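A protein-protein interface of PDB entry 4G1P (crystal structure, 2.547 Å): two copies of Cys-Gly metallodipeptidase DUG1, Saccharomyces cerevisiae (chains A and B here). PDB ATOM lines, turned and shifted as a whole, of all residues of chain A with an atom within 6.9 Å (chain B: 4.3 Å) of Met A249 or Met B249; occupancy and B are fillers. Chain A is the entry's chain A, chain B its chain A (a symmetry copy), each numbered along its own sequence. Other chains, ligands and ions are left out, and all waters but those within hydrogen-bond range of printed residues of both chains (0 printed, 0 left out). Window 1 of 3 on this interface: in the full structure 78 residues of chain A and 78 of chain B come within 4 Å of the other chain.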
ATOM      1  N   ILE A 225      15.491  -7.907  18.521  1.00  0.00           N
ATOM      2  CA  ILE A 225      16.357  -7.933  17.348  1.00  0.00           C
ATOM      3  C   ILE A 225      17.712  -7.325  17.685  1.00  0.00           C
ATOM      4  O   ILE A 225      17.795  -6.187  18.166  1.00  0.00           O
ATOM      5  CB  ILE A 225      15.740  -7.181  16.175  1.00  0.00           C
ATOM      6  CG1 ILE A 225      14.427  -7.834  15.763  1.00  0.00           C
ATOM      7  CG2 ILE A 225      16.685  -7.178  14.991  1.00  0.00           C
ATOM      8  CD1 ILE A 225      13.705  -7.098  14.653  1.00  0.00           C
ATOM      9  N   PRO A 244      18.870  -3.210  13.216  1.00  0.00           N
ATOM     10  CA  PRO A 244      17.801  -3.821  14.007  1.00  0.00           C
ATOM     11  C   PRO A 244      16.516  -2.984  14.006  1.00  0.00           C
ATOM     12  O   PRO A 244      15.438  -3.543  13.830  1.00  0.00           O
ATOM     13  CB  PRO A 244      18.410  -3.884  15.403  1.00  0.00           C
ATOM     14  CG  PRO A 244      19.854  -4.083  15.143  1.00  0.00           C
ATOM     15  CD  PRO A 244      20.167  -3.274  13.910  1.00  0.00           C
ATOM     16  N   MET A 245      16.631  -1.670  14.162  1.00  0.00           N
ATOM     17  CA  MET A 245      15.451  -0.813  14.109  1.00  0.00           C
ATOM     18  C   MET A 245      14.664  -0.919  12.800  1.00  0.00           C
ATOM     19  O   MET A 245      13.435  -0.813  12.801  1.00  0.00           O
ATOM     20  CB  MET A 245      15.801   0.649  14.407  1.00  0.00           C
ATOM     21  CG  MET A 245      15.796   0.990  15.893  1.00  0.00           C
ATOM     22  SD  MET A 245      14.237   0.640  16.767  1.00  0.00           S
ATOM     23  CE  MET A 245      13.185   1.942  16.130  1.00  0.00           C
ATOM     24  N   ILE A 246      15.363  -1.128  11.691  1.00  0.00           N
ATOM     25  CA  ILE A 246      14.702  -1.188  10.397  1.00  0.00           C
ATOM     26  C   ILE A 246      13.919  -2.501  10.260  1.00  0.00           C
ATOM     27  O   ILE A 246      12.746  -2.509   9.871  1.00  0.00           O
ATOM     28  CB  ILE A 246      15.703  -0.984   9.259  1.00  0.00           C
ATOM     29  CG1 ILE A 246      16.221   0.455   9.287  1.00  0.00           C
ATOM     30  CG2 ILE A 246      15.065  -1.272   7.922  1.00  0.00           C
ATOM     31  CD1 ILE A 246      17.368   0.736   8.319  1.00  0.00           C
ATOM     32  N   ASP A 247      14.562  -3.608  10.607  1.00  0.00           N
ATOM     33  CA  ASP A 247      13.863  -4.885  10.638  1.00  0.00           C
ATOM     34  C   ASP A 247      12.642  -4.793  11.550  1.00  0.00           C
ATOM     35  O   ASP A 247      11.538  -5.219  11.180  1.00  0.00           O
ATOM     36  CB  ASP A 247      14.796  -5.997  11.111  1.00  0.00           C
ATOM     37  CG  ASP A 247      16.039  -6.118  10.242  1.00  0.00           C
ATOM     38  OD1 ASP A 247      15.999  -5.606   9.106  1.00  0.00           O
ATOM     39  OD2 ASP A 247      17.044  -6.716  10.692  1.00  0.00           O
ATOM     40  N   LEU A 248      12.844  -4.201  12.724  1.00  0.00           N
ATOM     41  CA  LEU A 248      11.817  -4.142  13.757  1.00  0.00           C
ATOM     42  C   LEU A 248      10.559  -3.396  13.332  1.00  0.00           C
ATOM     43  O   LEU A 248       9.459  -3.796  13.696  1.00  0.00           O
ATOM     44  CB  LEU A 248      12.371  -3.540  15.048  1.00  0.00           C
ATOM     45  CG  LEU A 248      11.371  -3.597  16.206  1.00  0.00           C
ATOM     46  CD1 LEU A 248      11.200  -5.040  16.655  1.00  0.00           C
ATOM     47  CD2 LEU A 248      11.737  -2.670  17.379  1.00  0.00           C
ATOM     48  N   MET A 249      10.707  -2.319  12.569  1.00  0.00           N
ATOM     49  CA  MET A 249       9.534  -1.619  12.067  1.00  0.00           C
ATOM     50  C   MET A 249       8.733  -2.525  11.147  1.00  0.00           C
ATOM     51  O   MET A 249       7.503  -2.470  11.101  1.00  0.00           O
ATOM     52  CB  MET A 249       9.924  -0.337  11.340  1.00  0.00           C
ATOM     53  CG  MET A 249      10.709   0.632  12.213  1.00  0.00           C
ATOM     54  SD  MET A 249       9.831   1.192  13.694  1.00  0.00           S
ATOM     55  CE  MET A 249      10.345   0.026  14.967  1.00  0.00           C
ATOM     56  N   GLN A 250       9.434  -3.379  10.422  1.00  0.00           N
ATOM     57  CA  GLN A 250       8.760  -4.291   9.530  1.00  0.00           C
ATOM     58  C   GLN A 250       8.063  -5.426  10.284  1.00  0.00           C
ATOM     59  O   GLN A 250       6.910  -5.735  10.013  1.00  0.00           O
ATOM     60  CB  GLN A 250       9.728  -4.783   8.450  1.00  0.00           C
ATOM     61  CG  GLN A 250       9.800  -3.793   7.298  1.00  0.00           C
ATOM     62  CD  GLN A 250      11.128  -3.785   6.570  1.00  0.00           C
ATOM     63  OE1 GLN A 250      11.981  -4.649   6.782  1.00  0.00           O
ATOM     64  NE2 GLN A 250      11.312  -2.795   5.698  1.00  0.00           N
ATOM     65  N   VAL A 251       8.747  -6.028  11.244  1.00  0.00           N
ATOM     66  CA  VAL A 251       8.149  -7.121  11.989  1.00  0.00           C
ATOM     67  C   VAL A 251       6.952  -6.628  12.792  1.00  0.00           C
ATOM     68  O   VAL A 251       5.868  -7.205  12.736  1.00  0.00           O
ATOM     69  CB  VAL A 251       9.176  -7.815  12.902  1.00  0.00           C
ATOM     70  CG1 VAL A 251       8.483  -8.743  13.875  1.00  0.00           C
ATOM     71  CG2 VAL A 251      10.178  -8.597  12.066  1.00  0.00           C
ATOM     72  N   LEU A 252       7.156  -5.539  13.519  1.00  0.00           N
ATOM     73  CA  LEU A 252       6.120  -4.957  14.360  1.00  0.00           C
ATOM     74  C   LEU A 252       4.961  -4.477  13.513  1.00  0.00           C
ATOM     75  O   LEU A 252       3.804  -4.578  13.908  1.00  0.00           O
ATOM     76  CB  LEU A 252       6.691  -3.775  15.135  1.00  0.00           C
ATOM     77  CG  LEU A 252       6.782  -3.858  16.653  1.00  0.00           C
ATOM     78  CD1 LEU A 252       6.805  -5.305  17.130  1.00  0.00           C
ATOM     79  CD2 LEU A 252       8.004  -3.092  17.131  1.00  0.00           C
ATOM     80  N   GLY A 253       5.281  -3.957  12.334  1.00  0.00           N
ATOM     81  CA  GLY A 253       4.282  -3.370  11.466  1.00  0.00           C
ATOM     82  C   GLY A 253       3.467  -4.411  10.724  1.00  0.00           C
ATOM     83  O   GLY A 253       2.667  -4.076   9.862  1.00  0.00           O
ATOM     84  N   SER A 254       3.658  -5.675  11.071  1.00  0.00           N
ATOM     85  CA  SER A 254       3.015  -6.758  10.355  1.00  0.00           C
ATOM     86  C   SER A 254       2.048  -7.472  11.275  1.00  0.00           C
ATOM     87  O   SER A 254       1.488  -8.507  10.910  1.00  0.00           O
ATOM     88  CB  SER A 254       4.059  -7.758   9.867  1.00  0.00           C
ATOM     89  OG  SER A 254       4.507  -8.571  10.943  1.00  0.00           O
ATOM     90  N   ILE A 321       0.367  -1.850  20.284  1.00  0.00           N
ATOM     91  CA  ILE A 321       1.818  -1.712  20.206  1.00  0.00           C
ATOM     92  C   ILE A 321       2.301  -0.589  21.126  1.00  0.00           C
ATOM     93  O   ILE A 321       1.932   0.565  20.953  1.00  0.00           O
ATOM     94  CB  ILE A 321       2.288  -1.566  18.747  1.00  0.00           C
ATOM     95  CG1 ILE A 321       2.089  -2.899  18.034  1.00  0.00           C
ATOM     96  CG2 ILE A 321       3.757  -1.169  18.683  1.00  0.00           C
ATOM     97  CD1 ILE A 321       2.388  -2.863  16.574  1.00  0.00           C
ATOM     98  N   VAL A 324       9.232   0.925  21.989  1.00  0.00           N
ATOM     99  CA  VAL A 324      10.487   0.245  21.728  1.00  0.00           C
ATOM    100  C   VAL A 324      11.467   0.494  22.860  1.00  0.00           C
ATOM    101  O   VAL A 324      11.637   1.632  23.297  1.00  0.00           O
ATOM    102  CB  VAL A 324      11.124   0.730  20.408  1.00  0.00           C
ATOM    103  CG1 VAL A 324      12.391  -0.020  20.146  1.00  0.00           C
ATOM    104  CG2 VAL A 324      10.180   0.527  19.270  1.00  0.00           C
ATOM    105  N   MET B 245       0.886   4.472  17.594  1.00  0.00           N
ATOM    106  CA  MET B 245       1.985   3.525  17.438  1.00  0.00           C
ATOM    107  C   MET B 245       1.814   2.560  16.261  1.00  0.00           C
ATOM    108  O   MET B 245       2.795   2.178  15.620  1.00  0.00           O
ATOM    109  CB  MET B 245       2.251   2.749  18.733  1.00  0.00           C
ATOM    110  CG  MET B 245       3.199   3.461  19.691  1.00  0.00           C
ATOM    111  SD  MET B 245       4.829   3.889  18.999  1.00  0.00           S
ATOM    112  CE  MET B 245       5.601   2.276  18.913  1.00  0.00           C
ATOM    113  N   ILE B 246       0.577   2.169  15.977  1.00  0.00           N
ATOM    114  CA  ILE B 246       0.327   1.212  14.911  1.00  0.00           C
ATOM    115  C   ILE B 246       0.529   1.877  13.543  1.00  0.00           C
ATOM    116  O   ILE B 246       1.213   1.339  12.665  1.00  0.00           O
ATOM    117  CB  ILE B 246      -1.059   0.579  15.055  1.00  0.00           C
ATOM    118  CG1 ILE B 246      -1.086  -0.311  16.297  1.00  0.00           C
ATOM    119  CG2 ILE B 246      -1.408  -0.234  13.834  1.00  0.00           C
ATOM    120  CD1 ILE B 246      -2.467  -0.853  16.660  1.00  0.00           C
ATOM    121  N   ASP B 247      -0.046   3.060  13.373  1.00  0.00           N
ATOM    122  CA  ASP B 247       0.197   3.828  12.160  1.00  0.00           C
ATOM    123  C   ASP B 247       1.696   4.046  11.967  1.00  0.00           C
ATOM    124  O   ASP B 247       2.232   3.840  10.870  1.00  0.00           O
ATOM    125  CB  ASP B 247      -0.532   5.168  12.218  1.00  0.00           C
ATOM    126  CG  ASP B 247      -2.031   5.004  12.425  1.00  0.00           C
ATOM    127  OD1 ASP B 247      -2.528   3.891  12.166  1.00  0.00           O
ATOM    128  OD2 ASP B 247      -2.700   5.977  12.844  1.00  0.00           O
ATOM    129  N   LEU B 248       2.365   4.426  13.052  1.00  0.00           N
ATOM    130  CA  LEU B 248       3.775   4.796  13.012  1.00  0.00           C
ATOM    131  C   LEU B 248       4.692   3.669  12.553  1.00  0.00           C
ATOM    132  O   LEU B 248       5.658   3.918  11.840  1.00  0.00           O
ATOM    133  CB  LEU B 248       4.241   5.332  14.365  1.00  0.00           C
ATOM    134  CG  LEU B 248       5.674   5.871  14.326  1.00  0.00           C
ATOM    135  CD1 LEU B 248       5.706   7.161  13.520  1.00  0.00           C
ATOM    136  CD2 LEU B 248       6.299   6.050  15.721  1.00  0.00           C
ATOM    137  N   MET B 249       4.404   2.435  12.954  1.00  0.00           N
ATOM    138  CA  MET B 249       5.200   1.313  12.477  1.00  0.00           C
ATOM    139  C   MET B 249       5.064   1.174  10.970  1.00  0.00           C
ATOM    140  O   MET B 249       6.006   0.798  10.271  1.00  0.00           O
ATOM    141  CB  MET B 249       4.795   0.017  13.167  1.00  0.00           C
ATOM    142  CG  MET B 249       4.932   0.076  14.682  1.00  0.00           C
ATOM    143  SD  MET B 249       6.610   0.410  15.275  1.00  0.00           S
ATOM    144  CE  MET B 249       6.657   2.201  15.454  1.00  0.00           C
ATOM    145  N   GLN B 250       3.887   1.498  10.462  1.00  0.00           N
ATOM    146  CA  GLN B 250       3.667   1.412   9.039  1.00  0.00           C
ATOM    147  C   GLN B 250       4.361   2.544   8.278  1.00  0.00           C
ATOM    148  O   GLN B 250       5.023   2.305   7.276  1.00  0.00           O
ATOM    149  CB  GLN B 250       2.169   1.311   8.743  1.00  0.00           C
ATOM    150  CG  GLN B 250       1.692  -0.129   8.849  1.00  0.00           C
ATOM    151  CD  GLN B 250       0.242  -0.273   9.259  1.00  0.00           C
ATOM    152  OE1 GLN B 250      -0.513   0.699   9.301  1.00  0.00           O
ATOM    153  NE2 GLN B 250      -0.158  -1.506   9.571  1.00  0.00           N
ATOM    154  N   VAL B 251       4.236   3.770   8.765  1.00  0.00           N
ATOM    155  CA  VAL B 251       4.859   4.890   8.084  1.00  0.00           C
ATOM    156  C   VAL B 251       6.376   4.754   8.111  1.00  0.00           C
ATOM    157  O   VAL B 251       7.042   4.864   7.083  1.00  0.00           O
ATOM    158  CB  VAL B 251       4.416   6.236   8.686  1.00  0.00           C
ATOM    159  CG1 VAL B 251       5.286   7.362   8.171  1.00  0.00           C
ATOM    160  CG2 VAL B 251       2.960   6.511   8.343  1.00  0.00           C
ATOM    161  N   LEU B 252       6.909   4.489   9.294  1.00  0.00           N
ATOM    162  CA  LEU B 252       8.346   4.353   9.490  1.00  0.00           C
ATOM    163  C   LEU B 252       8.876   3.171   8.708  1.00  0.00           C
ATOM    164  O   LEU B 252       9.978   3.211   8.170  1.00  0.00           O
ATOM    165  CB  LEU B 252       8.645   4.142  10.970  1.00  0.00           C
ATOM    166  CG  LEU B 252       9.432   5.205  11.726  1.00  0.00           C
ATOM    167  CD1 LEU B 252       9.329   6.563  11.043  1.00  0.00           C
ATOM    168  CD2 LEU B 252       8.950   5.265  13.165  1.00  0.00           C
ATOM    169  N   GLY B 253       8.075   2.115   8.641  1.00  0.00           N
ATOM    170  CA  GLY B 253       8.495   0.881   8.008  1.00  0.00           C
ATOM    171  C   GLY B 253       8.439   0.950   6.496  1.00  0.00           C
ATOM    172  O   GLY B 253       8.645  -0.048   5.819  1.00  0.00           O
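SD of Met A249 sits close to SD of Met B249.
Gly B253 touches Met A249 (CA to CB, 3.8 Å).
Gly B253 touches Gln A250 (O to NE2, 3.8 Å).
Gly A253 touches Met B249.
Gln B250 touches Gly A253 (NE2 to O, 3.8 Å).
Met B245 touches Ile A321.
Met A249 touches two residues of chain B.
Printed residues of chain B within 4 Å of Gln A250: Gly B253 (3.8 Å).
Printed residues of chain B within 4 Å of Gly A253: Met B249 and Gln B250.
Met B249 touches just these residues of chain A: Met A249 and Gly A253.
Of the printed residues of chain A, Gln B250 touches Gly A253 (3.8 Å).
Of the printed residues of chain A, Gly B253 touches Met A249 and Gln A250.
The nearest residue of chain B that does not touch Met A249 is Leu B252 (4.2 Å).
The nearest residue of chain A that does not touch Met B249 is Leu A252 (4.2 Å).
Of the 9 printed residues of chain B, 4 touch a printed residue of chain A.
Met A249 touches its own counterpart, Met B249.
Met A249 touches Gly B253, and with the chains exchanged Gly A253 touches Met B249.
Gln A250 touches Gly B253, and with the chains exchanged Gly A253 touches Gln B250.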
